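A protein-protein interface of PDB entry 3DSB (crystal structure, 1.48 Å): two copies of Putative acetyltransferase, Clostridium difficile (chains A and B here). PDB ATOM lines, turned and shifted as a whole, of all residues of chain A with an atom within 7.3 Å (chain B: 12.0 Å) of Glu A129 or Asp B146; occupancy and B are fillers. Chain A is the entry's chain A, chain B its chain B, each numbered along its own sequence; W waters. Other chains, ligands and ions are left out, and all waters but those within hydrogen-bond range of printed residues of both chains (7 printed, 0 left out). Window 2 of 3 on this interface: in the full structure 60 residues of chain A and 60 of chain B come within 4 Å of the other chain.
The backbone NH (N) of Lys A128 is in hydrogen-bond range of the backbone carbonyl oxygen (O) of Asp B146, at 3.0 Å. OE1 of Glu A151 lies within salt-bridge range of NE of Arg B123, 3.1 Å away. The backbone NH (N) of Asn B148 is in hydrogen-bond range of the backbone carbonyl oxygen (O) of Val A126. OE2 of Glu A129 sits close to OD2 of Asp B146. O of Met A149 is in hydrogen-bond range of N of Cys B145 (2.8 Å). N of Glu A151 is in hydrogen-bond range of O of Tyr B143 (2.9 Å). The backbone NH (N) of Glu A151 lies close to the side-chain sulfur (SG) of Cys B145, at 3.7 Å.
CE2 of Tyr B150 touches CG1 of Val A126, at 3.6 Å. Glu A127 touches Asp B146 (CA to O, 3.5 Å). Lys A128 touches Cys B145 (NZ to O, 3.9 Å). Lys A128 touches Tyr B147. Met A149 touches Trp B86 (CE to CH2, 3.7 Å). Met A149 touches Leu B124 (CA to O, 3.2 Å). Met A149 touches Glu B144. Met A149 touches Tyr B147 (CE to CD2, 3.1 Å). O of Met B122 touches CA of Glu A151 (3.2 Å). Glu A151 touches Met B142 (O to CA, 3.3 Å).
Water W2 lies within hydrogen-bond range of the side-chain carboxylate of Asp B146 and the side-chain carboxylate of Glu A129. Water W5 lies within hydrogen-bond range of OE2 of Glu B144 (2.6 Å), NZ of Lys A128 (2.6 Å) and O of Cys B145 (3.5 Å). Water W4 lies within hydrogen-bond range of the side-chain carboxylate of Glu A151 (2.7 Å), the side-chain hydroxyl of Tyr B147 (3.3 Å) and the guanidinium group of Arg B123 (3.3 Å). Water W7 lies within hydrogen-bond range of the side-chain amino group of Lys A128 (2.8 Å) and the side-chain carboxylate of Asp B146 (3.4 Å). Water W1 lies within hydrogen-bond range of the side-chain carboxylate of Glu A151 (2.8 Å) and the guanidinium group of Arg B123 (3.3 Å). Water W6 lies within hydrogen-bond range of N of Met B122 and OE1 of Glu A151.
3 positions are printed for both chains.
The side-chain carboxylate (OE1) of Glu B144 lies within salt-bridge range of the side-chain amino group (NZ) of Lys B134 (2.5 Å). NH2 of Arg B123 is in hydrogen-bond range of OH of Tyr B147 (3.5 Å).
Hydrophobic or aromatic side chains of chain B that line the printed part of chain A: Trp B86, Met B142, Tyr B147 and Tyr B150. Of the 10 printed residues of chain A, 6 touch a printed residue of chain B.
Val A126 touches just these residues of chain B: Tyr B147 (3.3 Å), Asn B148 (2.9 Å) and Tyr B150 (3.6 Å). Of chain B, only Asp B146 (3.5 Å) and Tyr B147 (3.7 Å) come within 4 Å of Glu A127. Lys A128 touches four residues of chain B. Printed residues of chain B within 4 Å of Glu A129: Asp B146. Asn A132 touches none of the printed residues of chain B. Met A149 touches just these residues of chain B: Trp B86 (3.7 Å), Leu B124 (3.2 Å), Glu B144 (3.4 Å), Cys B145 (2.8 Å) and Tyr B147 (3.1 Å). Arg B80 touches none of the printed residues of chain A. Printed residues of chain A within 4 Å of Arg B123: Glu A151. Of the printed residues of chain A, Tyr B143 touches Glu A151. Of the printed residues of chain A, Asp B146 touches Glu A127, Lys A128 and Glu A129. The nearest printed residue of chain A that does not touch Tyr B150 is Ala A133 (4.5 Å).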
ATOM      1  N   VAL A 126     -12.610   0.955  -5.161  1.00  0.00           N
ATOM      2  CA  VAL A 126     -13.941   0.547  -4.734  1.00  0.00           C
ATOM      3  C   VAL A 126     -15.013   1.400  -5.395  1.00  0.00           C
ATOM      4  O   VAL A 126     -14.786   2.576  -5.686  1.00  0.00           O
ATOM      5  CB  VAL A 126     -14.035   0.618  -3.178  1.00  0.00           C
ATOM      6  CG1 VAL A 126     -13.825   2.054  -2.634  1.00  0.00           C
ATOM      7  CG2 VAL A 126     -15.346   0.003  -2.658  1.00  0.00           C
ATOM      8  N   GLU A 127     -16.170   0.808  -5.648  1.00  0.00           N
ATOM      9  CA  GLU A 127     -17.270   1.579  -6.229  1.00  0.00           C
ATOM     10  C   GLU A 127     -17.579   2.809  -5.402  1.00  0.00           C
ATOM     11  O   GLU A 127     -17.613   2.737  -4.164  1.00  0.00           O
ATOM     12  CB  GLU A 127     -18.551   0.728  -6.283  1.00  0.00           C
ATOM     13  CG  GLU A 127     -18.549  -0.375  -7.250  1.00  0.00           C
ATOM     14  CD  GLU A 127     -19.843  -1.225  -7.190  1.00  0.00           C
ATOM     15  OE1 GLU A 127     -20.724  -0.933  -6.361  1.00  0.00           O
ATOM     16  OE2 GLU A 127     -19.937  -2.196  -7.961  1.00  0.00           O
ATOM     17  N   LYS A 128     -17.892   3.918  -6.076  1.00  0.00           N
ATOM     18  CA  LYS A 128     -18.236   5.160  -5.357  1.00  0.00           C
ATOM     19  C   LYS A 128     -19.530   4.992  -4.541  1.00  0.00           C
ATOM     20  O   LYS A 128     -19.730   5.692  -3.556  1.00  0.00           O
ATOM     21  CB  LYS A 128     -18.408   6.351  -6.321  1.00  0.00           C
ATOM     22  CG  LYS A 128     -17.119   6.745  -7.010  1.00  0.00           C
ATOM     23  CD  LYS A 128     -17.320   7.952  -7.911  1.00  0.00           C
ATOM     24  CE  LYS A 128     -15.988   8.354  -8.559  1.00  0.00           C
ATOM     25  NZ  LYS A 128     -16.179   9.360  -9.649  1.00  0.00           N
ATOM     26  N   GLU A 129     -20.375   4.066  -4.982  1.00  0.00           N
ATOM     27  CA  GLU A 129     -21.668   3.822  -4.321  1.00  0.00           C
ATOM     28  C   GLU A 129     -21.584   3.083  -3.009  1.00  0.00           C
ATOM     29  O   GLU A 129     -22.583   2.983  -2.278  1.00  0.00           O
ATOM     30  CB  GLU A 129     -22.624   3.065  -5.251  1.00  0.00           C
ATOM     31  CG  GLU A 129     -23.067   3.878  -6.422  1.00  0.00           C
ATOM     32  CD  GLU A 129     -22.102   3.814  -7.584  1.00  0.00           C
ATOM     33  OE1 GLU A 129     -21.077   3.078  -7.488  1.00  0.00           O
ATOM     34  OE2 GLU A 129     -22.378   4.514  -8.595  1.00  0.00           O
ATOM     35  N   ASN A 130     -20.424   2.525  -2.702  1.00  0.00           N
ATOM     36  CA  ASN A 130     -20.296   1.764  -1.490  1.00  0.00           C
ATOM     37  C   ASN A 130     -20.213   2.741  -0.348  1.00  0.00           C
ATOM     38  O   ASN A 130     -19.161   3.313  -0.099  1.00  0.00           O
ATOM     39  CB  ASN A 130     -19.061   0.879  -1.573  1.00  0.00           C
ATOM     40  CG  ASN A 130     -18.939  -0.053  -0.397  1.00  0.00           C
ATOM     41  OD1 ASN A 130     -19.208   0.323   0.756  1.00  0.00           O
ATOM     42  ND2 ASN A 130     -18.490  -1.270  -0.675  1.00  0.00           N
ATOM     43  N   ILE A 131     -21.343   2.898   0.351  1.00  0.00           N
ATOM     44  CA  ILE A 131     -21.522   3.907   1.407  1.00  0.00           C
ATOM     45  C   ILE A 131     -20.682   3.651   2.664  1.00  0.00           C
ATOM     46  O   ILE A 131     -20.432   4.586   3.433  1.00  0.00           O
ATOM     47  CB  ILE A 131     -23.040   4.099   1.796  1.00  0.00           C
ATOM     48  CG1 ILE A 131     -23.631   2.838   2.472  1.00  0.00           C
ATOM     49  CG2 ILE A 131     -23.850   4.543   0.574  1.00  0.00           C
ATOM     50  CD1 ILE A 131     -25.077   2.997   2.998  1.00  0.00           C
ATOM     51  N   ASN A 132     -20.221   2.412   2.843  1.00  0.00           N
ATOM     52  CA  ASN A 132     -19.543   2.008   4.068  1.00  0.00           C
ATOM     53  C   ASN A 132     -18.027   1.868   3.949  1.00  0.00           C
ATOM     54  O   ASN A 132     -17.333   1.738   4.958  1.00  0.00           O
ATOM     55  CB  ASN A 132     -20.139   0.708   4.574  1.00  0.00           C
ATOM     56  CG  ASN A 132     -21.621   0.829   4.868  1.00  0.00           C
ATOM     57  OD1 ASN A 132     -22.431   0.119   4.282  1.00  0.00           O
ATOM     58  ND2 ASN A 132     -21.981   1.754   5.743  1.00  0.00           N
ATOM     59  N   ALA A 133     -17.541   1.923   2.709  1.00  0.00           N
ATOM     60  CA  ALA A 133     -16.093   1.736   2.426  1.00  0.00           C
ATOM     61  C   ALA A 133     -15.230   2.768   3.121  1.00  0.00           C
ATOM     62  O   ALA A 133     -14.248   2.422   3.770  1.00  0.00           O
ATOM     63  CB  ALA A 133     -15.810   1.763   0.899  1.00  0.00           C
ATOM     64  N   MET A 149     -10.056   7.140 -12.168  1.00  0.00           N
ATOM     65  CA  MET A 149      -9.722   6.042 -13.063  1.00  0.00           C
ATOM     66  C   MET A 149     -10.452   6.254 -14.396  1.00  0.00           C
ATOM     67  O   MET A 149     -11.579   6.791 -14.409  1.00  0.00           O
ATOM     68  CB  MET A 149     -10.142   4.739 -12.421  1.00  0.00           C
ATOM     69  CG  MET A 149      -9.095   4.265 -11.432  1.00  0.00           C
ATOM     70  SD  MET A 149      -9.688   2.750 -10.401  1.00  0.00           S
ATOM     71  CE  MET A 149     -10.645   1.837 -11.962  1.00  0.00           C
ATOM     72  N   GLU A 151     -11.304   4.164 -18.321  1.00  0.00           N
ATOM     73  CA  GLU A 151     -11.196   2.859 -18.964  1.00  0.00           C
ATOM     74  C   GLU A 151     -11.688   2.892 -20.393  1.00  0.00           C
ATOM     75  O   GLU A 151     -12.542   3.735 -20.772  1.00  0.00           O
ATOM     76  CB  GLU A 151     -11.942   1.802 -18.168  1.00  0.00           C
ATOM     77  CG  GLU A 151     -13.435   1.859 -18.309  1.00  0.00           C
ATOM     78  CD  GLU A 151     -14.144   0.818 -17.459  1.00  0.00           C
ATOM     79  OE1 GLU A 151     -13.512  -0.217 -17.091  1.00  0.00           O
ATOM     80  OE2 GLU A 151     -15.369   0.981 -17.225  1.00  0.00           O
ATOM     81  N   ARG B  80     -13.136 -12.387 -13.809  1.00  0.00           N
ATOM     82  CA  ARG B  80     -13.315 -12.310 -15.268  1.00  0.00           C
ATOM     83  C   ARG B  80     -12.399 -13.266 -16.037  1.00  0.00           C
ATOM     84  O   ARG B  80     -12.465 -13.356 -17.282  1.00  0.00           O
ATOM     85  CB  ARG B  80     -13.040 -10.888 -15.723  1.00  0.00           C
ATOM     86  CG  ARG B  80     -14.070  -9.868 -15.186  1.00  0.00           C
ATOM     87  CD  ARG B  80     -13.650  -8.469 -15.599  1.00  0.00           C
ATOM     88  NE  ARG B  80     -14.532  -7.433 -15.078  1.00  0.00           N
ATOM     89  CZ  ARG B  80     -15.486  -6.873 -15.813  1.00  0.00           C
ATOM     90  NH1 ARG B  80     -15.675  -7.296 -17.066  1.00  0.00           N
ATOM     91  NH2 ARG B  80     -16.264  -5.923 -15.295  1.00  0.00           N
ATOM     92  N   PHE B  84      -6.669  -7.104 -16.702  1.00  0.00           N
ATOM     93  CA  PHE B  84      -6.788  -5.721 -17.130  1.00  0.00           C
ATOM     94  C   PHE B  84      -5.376  -5.264 -17.434  1.00  0.00           C
ATOM     95  O   PHE B  84      -4.450  -5.567 -16.693  1.00  0.00           O
ATOM     96  CB  PHE B  84      -7.319  -4.853 -15.986  1.00  0.00           C
ATOM     97  CG  PHE B  84      -8.741  -5.063 -15.683  1.00  0.00           C
ATOM     98  CD1 PHE B  84      -9.728  -4.390 -16.384  1.00  0.00           C
ATOM     99  CD2 PHE B  84      -9.116  -5.956 -14.649  1.00  0.00           C
ATOM    100  CE1 PHE B  84     -11.084  -4.581 -16.131  1.00  0.00           C
ATOM    101  CE2 PHE B  84     -10.454  -6.170 -14.374  1.00  0.00           C
ATOM    102  CZ  PHE B  84     -11.454  -5.474 -15.122  1.00  0.00           C
ATOM    103  N   TRP B  86      -3.131  -1.917 -17.332  1.00  0.00           N
ATOM    104  CA  TRP B  86      -3.132  -0.598 -16.688  1.00  0.00           C
ATOM    105  C   TRP B  86      -2.041   0.244 -17.311  1.00  0.00           C
ATOM    106  O   TRP B  86      -0.857  -0.075 -17.164  1.00  0.00           O
ATOM    107  CB  TRP B  86      -2.869  -0.760 -15.189  1.00  0.00           C
ATOM    108  CG  TRP B  86      -4.078  -1.209 -14.441  1.00  0.00           C
ATOM    109  CD1 TRP B  86      -4.532  -2.481 -14.298  1.00  0.00           C
ATOM    110  CD2 TRP B  86      -5.055  -0.348 -13.850  1.00  0.00           C
ATOM    111  NE1 TRP B  86      -5.717  -2.485 -13.544  1.00  0.00           N
ATOM    112  CE2 TRP B  86      -6.045  -1.181 -13.246  1.00  0.00           C
ATOM    113  CE3 TRP B  86      -5.118   1.033 -13.639  1.00  0.00           C
ATOM    114  CZ2 TRP B  86      -7.142  -0.649 -12.551  1.00  0.00           C
ATOM    115  CZ3 TRP B  86      -6.212   1.549 -12.960  1.00  0.00           C
ATOM    116  CH2 TRP B  86      -7.193   0.714 -12.403  1.00  0.00           C
ATOM    117  N   MET B 122      -8.997  -2.295 -19.992  1.00  0.00           N
ATOM    118  CA  MET B 122      -7.837  -1.424 -20.183  1.00  0.00           C
ATOM    119  C   MET B 122      -8.138  -0.184 -19.371  1.00  0.00           C
ATOM    120  O   MET B 122      -9.149   0.493 -19.609  1.00  0.00           O
ATOM    121  CB  MET B 122      -7.686  -1.054 -21.670  1.00  0.00           C
ATOM    122  CG  MET B 122      -6.469  -0.242 -21.915  1.00  0.00           C
ATOM    123  SD  MET B 122      -6.237   0.184 -23.786  1.00  0.00           S
ATOM    124  CE  MET B 122      -6.594   2.078 -23.586  1.00  0.00           C
ATOM    125  N   ARG B 123      -7.285   0.100 -18.382  1.00  0.00           N
ATOM    126  CA  ARG B 123      -7.578   1.172 -17.419  1.00  0.00           C
ATOM    127  C   ARG B 123      -6.332   2.009 -17.166  1.00  0.00           C
ATOM    128  O   ARG B 123      -5.219   1.605 -17.515  1.00  0.00           O
ATOM    129  CB  ARG B 123      -8.039   0.545 -16.099  1.00  0.00           C
ATOM    130  CG  ARG B 123      -9.365  -0.186 -16.249  1.00  0.00           C
ATOM    131  CD  ARG B 123      -9.882  -0.886 -14.978  1.00  0.00           C
ATOM    132  NE  ARG B 123     -11.304  -1.220 -15.138  1.00  0.00           N
ATOM    133  CZ  ARG B 123     -12.016  -1.962 -14.292  1.00  0.00           C
ATOM    134  NH1 ARG B 123     -11.451  -2.513 -13.229  1.00  0.00           N
ATOM    135  NH2 ARG B 123     -13.302  -2.199 -14.561  1.00  0.00           N
ATOM    136  N   LEU B 124      -6.552   3.161 -16.529  1.00  0.00           N
ATOM    137  CA  LEU B 124      -5.465   3.960 -15.996  1.00  0.00           C
ATOM    138  C   LEU B 124      -5.970   4.816 -14.849  1.00  0.00           C
ATOM    139  O   LEU B 124      -7.168   5.011 -14.715  1.00  0.00           O
ATOM    140  CB  LEU B 124      -4.812   4.848 -17.091  1.00  0.00           C
ATOM    141  CG  LEU B 124      -5.697   5.835 -17.830  1.00  0.00           C
ATOM    142  CD1 LEU B 124      -5.944   7.146 -17.040  1.00  0.00           C
ATOM    143  CD2 LEU B 124      -5.056   6.141 -19.167  1.00  0.00           C
ATOM    144  N   TYR B 125      -5.043   5.313 -14.028  1.00  0.00           N
ATOM    145  CA  TYR B 125      -5.409   6.325 -13.021  1.00  0.00           C
ATOM    146  C   TYR B 125      -4.589   7.571 -13.256  1.00  0.00           C
ATOM    147  O   TYR B 125      -3.436   7.482 -13.694  1.00  0.00           O
ATOM    148  CB  TYR B 125      -5.277   5.805 -11.556  1.00  0.00           C
ATOM    149  CG  TYR B 125      -3.875   5.324 -11.161  1.00  0.00           C
ATOM    150  CD1 TYR B 125      -2.909   6.232 -10.690  1.00  0.00           C
ATOM    151  CD2 TYR B 125      -3.513   3.993 -11.328  1.00  0.00           C
ATOM    152  CE1 TYR B 125      -1.610   5.830 -10.350  1.00  0.00           C
ATOM    153  CE2 TYR B 125      -2.255   3.557 -10.941  1.00  0.00           C
ATOM    154  CZ  TYR B 125      -1.278   4.500 -10.488  1.00  0.00           C
ATOM    155  OH  TYR B 125       0.048   4.148 -10.158  1.00  0.00           O
ATOM    156  N   VAL B 126      -5.218   8.729 -13.018  1.00  0.00           N
ATOM    157  CA  VAL B 126      -4.577  10.008 -13.203  1.00  0.00           C
ATOM    158  C   VAL B 126      -5.021  10.979 -12.099  1.00  0.00           C
ATOM    159  O   VAL B 126      -6.116  10.872 -11.559  1.00  0.00           O
ATOM    160  CB  VAL B 126      -4.975  10.569 -14.583  1.00  0.00           C
ATOM    161  CG1 VAL B 126      -6.488  10.746 -14.705  1.00  0.00           C
ATOM    162  CG2 VAL B 126      -4.233  11.868 -14.957  1.00  0.00           C
ATOM    163  N   LYS B 128      -6.527  13.887 -10.084  1.00  0.00           N
ATOM    164  CA  LYS B 128      -7.731  14.701 -10.347  1.00  0.00           C
ATOM    165  C   LYS B 128      -7.398  16.127 -10.825  1.00  0.00           C
ATOM    166  O   LYS B 128      -8.193  16.697 -11.551  1.00  0.00           O
ATOM    167  CB  LYS B 128      -8.643  14.789  -9.112  1.00  0.00           C
ATOM    168  CG  LYS B 128      -9.114  13.425  -8.609  1.00  0.00           C
ATOM    169  CD  LYS B 128      -9.946  13.583  -7.332  1.00  0.00           C
ATOM    170  CE  LYS B 128     -10.584  12.246  -6.903  1.00  0.00           C
ATOM    171  NZ  LYS B 128     -10.970  12.224  -5.464  1.00  0.00           N
ATOM    172  N   LYS B 134      -9.264  14.549 -18.897  1.00  0.00           N
ATOM    173  CA  LYS B 134     -10.585  14.126 -19.369  1.00  0.00           C
ATOM    174  C   LYS B 134     -10.722  14.255 -20.895  1.00  0.00           C
ATOM    175  O   LYS B 134     -11.109  13.306 -21.558  1.00  0.00           O
ATOM    176  CB  LYS B 134     -11.701  14.896 -18.662  1.00  0.00           C
ATOM    177  CG  LYS B 134     -13.095  14.389 -18.999  1.00  0.00           C
ATOM    178  CD  LYS B 134     -14.132  15.007 -18.065  1.00  0.00           C
ATOM    179  CE  LYS B 134     -14.931  13.890 -17.403  1.00  0.00           C
ATOM    180  NZ  LYS B 134     -14.015  12.879 -16.759  1.00  0.00           N
ATOM    181  N   GLU B 138     -11.039  11.170 -23.423  1.00  0.00           N
ATOM    182  CA  GLU B 138     -12.269  11.233 -24.191  1.00  0.00           C
ATOM    183  C   GLU B 138     -12.073  11.077 -25.694  1.00  0.00           C
ATOM    184  O   GLU B 138     -12.806  10.326 -26.334  1.00  0.00           O
ATOM    185  CB  GLU B 138     -13.004  12.544 -23.904  1.00  0.00           C
ATOM    186  CG  GLU B 138     -14.343  12.363 -23.220  1.00  0.00           C
ATOM    187  CD  GLU B 138     -14.253  12.107 -21.715  1.00  0.00           C
ATOM    188  OE1 GLU B 138     -15.265  12.421 -21.021  1.00  0.00           O
ATOM    189  OE2 GLU B 138     -13.200  11.596 -21.218  1.00  0.00           O
ATOM    190  N   MET B 142     -11.887   6.721 -24.037  1.00  0.00           N
ATOM    191  CA  MET B 142     -11.666   6.284 -22.656  1.00  0.00           C
ATOM    192  C   MET B 142     -12.386   7.252 -21.752  1.00  0.00           C
ATOM    193  O   MET B 142     -12.285   8.479 -21.916  1.00  0.00           O
ATOM    194  CB  MET B 142     -10.191   6.289 -22.317  1.00  0.00           C
ATOM    195  CG  MET B 142      -9.458   5.364 -23.196  1.00  0.00           C
ATOM    196  SD  MET B 142      -7.598   5.264 -22.698  1.00  0.00           S
ATOM    197  CE  MET B 142      -7.872   4.990 -20.872  1.00  0.00           C
ATOM    198  N   TYR B 143     -13.153   6.682 -20.816  1.00  0.00           N
ATOM    199  CA  TYR B 143     -14.057   7.479 -20.005  1.00  0.00           C
ATOM    200  C   TYR B 143     -13.858   7.193 -18.549  1.00  0.00           C
ATOM    201  O   TYR B 143     -13.385   6.137 -18.157  1.00  0.00           O
ATOM    202  CB  TYR B 143     -15.521   7.201 -20.405  1.00  0.00           C
ATOM    203  CG  TYR B 143     -15.724   7.424 -21.876  1.00  0.00           C
ATOM    204  CD1 TYR B 143     -15.655   8.698 -22.381  1.00  0.00           C
ATOM    205  CD2 TYR B 143     -15.971   6.353 -22.761  1.00  0.00           C
ATOM    206  CE1 TYR B 143     -15.824   8.959 -23.758  1.00  0.00           C
ATOM    207  CE2 TYR B 143     -16.146   6.594 -24.167  1.00  0.00           C
ATOM    208  CZ  TYR B 143     -16.050   7.896 -24.627  1.00  0.00           C
ATOM    209  OH  TYR B 143     -16.202   8.157 -25.991  1.00  0.00           O
ATOM    210  N   GLU B 144     -14.259   8.152 -17.733  1.00  0.00           N
ATOM    211  CA  GLU B 144     -14.061   8.050 -16.313  1.00  0.00           C
ATOM    212  C   GLU B 144     -14.905   6.945 -15.704  1.00  0.00           C
ATOM    213  O   GLU B 144     -16.111   6.790 -16.010  1.00  0.00           O
ATOM    214  CB  GLU B 144     -14.448   9.393 -15.706  1.00  0.00           C
ATOM    215  CG  GLU B 144     -14.067   9.515 -14.285  1.00  0.00           C
ATOM    216  CD  GLU B 144     -14.158  10.953 -13.777  1.00  0.00           C
ATOM    217  OE1 GLU B 144     -14.516  11.876 -14.540  1.00  0.00           O
ATOM    218  OE2 GLU B 144     -13.856  11.154 -12.610  1.00  0.00           O
ATOM    219  N   CYS B 145     -14.266   6.179 -14.823  1.00  0.00           N
ATOM    220  CA  CYS B 145     -14.919   5.097 -14.099  1.00  0.00           C
ATOM    221  C   CYS B 145     -15.556   5.570 -12.818  1.00  0.00           C
ATOM    222  O   CYS B 145     -15.371   6.713 -12.414  1.00  0.00           O
ATOM    223  CB  CYS B 145     -13.899   4.031 -13.726  1.00  0.00           C
ATOM    224  SG  CYS B 145     -12.922   3.365 -15.041  1.00  0.00           S
ATOM    225  N   ASP B 146     -16.332   4.690 -12.215  1.00  0.00           N
ATOM    226  CA  ASP B 146     -17.142   5.024 -11.038  1.00  0.00           C
ATOM    227  C   ASP B 146     -16.499   4.435  -9.795  1.00  0.00           C
ATOM    228  O   ASP B 146     -17.173   3.763  -8.995  1.00  0.00           O
ATOM    229  CB  ASP B 146     -18.574   4.470 -11.237  1.00  0.00           C
ATOM    230  CG  ASP B 146     -19.584   4.943 -10.186  1.00  0.00           C
ATOM    231  OD1 ASP B 146     -19.395   5.987  -9.549  1.00  0.00           O
ATOM    232  OD2 ASP B 146     -20.627   4.253 -10.082  1.00  0.00           O
ATOM    233  N   TYR B 147     -15.185   4.672  -9.656  1.00  0.00           N
ATOM    234  CA  TYR B 147     -14.436   4.144  -8.519  1.00  0.00           C
ATOM    235  C   TYR B 147     -13.639   5.213  -7.795  1.00  0.00           C
ATOM    236  O   TYR B 147     -13.192   6.195  -8.392  1.00  0.00           O
ATOM    237  CB  TYR B 147     -13.381   3.136  -8.957  1.00  0.00           C
ATOM    238  CG  TYR B 147     -13.894   1.942  -9.686  1.00  0.00           C
ATOM    239  CD1 TYR B 147     -14.611   0.933  -9.039  1.00  0.00           C
ATOM    240  CD2 TYR B 147     -13.601   1.799 -11.029  1.00  0.00           C
ATOM    241  CE1 TYR B 147     -15.101  -0.168  -9.739  1.00  0.00           C
ATOM    242  CE2 TYR B 147     -14.049   0.687 -11.739  1.00  0.00           C
ATOM    243  CZ  TYR B 147     -14.800  -0.273 -11.095  1.00  0.00           C
ATOM    244  OH  TYR B 147     -15.238  -1.352 -11.827  1.00  0.00           O
ATOM    245  N   ASN B 148     -13.480   5.009  -6.489  1.00  0.00           N
ATOM    246  CA  ASN B 148     -12.455   5.735  -5.729  1.00  0.00           C
ATOM    247  C   ASN B 148     -11.294   4.812  -5.404  1.00  0.00           C
ATOM    248  O   ASN B 148     -11.497   3.631  -5.176  1.00  0.00           O
ATOM    249  CB  ASN B 148     -13.044   6.261  -4.403  1.00  0.00           C
ATOM    250  CG  ASN B 148     -14.166   7.251  -4.628  1.00  0.00           C
ATOM    251  OD1 ASN B 148     -14.121   8.029  -5.589  1.00  0.00           O
ATOM    252  ND2 ASN B 148     -15.205   7.166  -3.807  1.00  0.00           N
ATOM    253  N   MET B 149     -10.082   5.372  -5.401  1.00  0.00           N
ATOM    254  CA  MET B 149      -8.906   4.648  -4.923  1.00  0.00           C
ATOM    255  C   MET B 149      -8.626   5.002  -3.473  1.00  0.00           C
ATOM    256  O   MET B 149      -8.873   6.147  -3.040  1.00  0.00           O
ATOM    257  CB  MET B 149      -7.717   4.957  -5.807  1.00  0.00           C
ATOM    258  CG  MET B 149      -7.726   4.149  -7.072  1.00  0.00           C
ATOM    259  SD  MET B 149      -6.292   4.701  -8.291  1.00  0.00           S
ATOM    260  CE  MET B 149      -4.964   5.117  -6.995  1.00  0.00           C
ATOM    261  N   TYR B 150      -8.121   4.012  -2.735  1.00  0.00           N
ATOM    262  CA  TYR B 150      -7.677   4.208  -1.356  1.00  0.00           C
ATOM    263  C   TYR B 150      -6.249   3.713  -1.221  1.00  0.00           C
ATOM    264  O   TYR B 150      -5.837   2.788  -1.947  1.00  0.00           O
ATOM    265  CB  TYR B 150      -8.551   3.414  -0.368  1.00  0.00           C
ATOM    266  CG  TYR B 150      -9.881   4.086  -0.124  1.00  0.00           C
ATOM    267  CD1 TYR B 150     -10.100   4.836   1.032  1.00  0.00           C
ATOM    268  CD2 TYR B 150     -10.928   3.976  -1.038  1.00  0.00           C
ATOM    269  CE1 TYR B 150     -11.301   5.502   1.260  1.00  0.00           C
ATOM    270  CE2 TYR B 150     -12.140   4.632  -0.824  1.00  0.00           C
ATOM    271  CZ  TYR B 150     -12.320   5.388   0.338  1.00  0.00           C
ATOM    272  OH  TYR B 150     -13.524   6.045   0.604  1.00  0.00           O
HETATM  273  O   HOH W   1     -15.077  -2.553 -17.376  1.00  0.00           O
HETATM  274  O   HOH W   2     -21.230   7.526  -8.645  1.00  0.00           O
HETATM  275  O   HOH W   3     -12.788   6.837 -11.034  1.00  0.00           O
HETATM  276  O   HOH W   4     -15.680   0.026 -14.743  1.00  0.00           O
HETATM  277  O   HOH W   5     -13.832   9.358 -10.777  1.00  0.00           O
HETATM  278  O   HOH W   6     -11.812  -1.738 -19.466  1.00  0.00           O
HETATM  279  O   HOH W   7     -18.207   8.608 -11.397  1.00  0.00           O
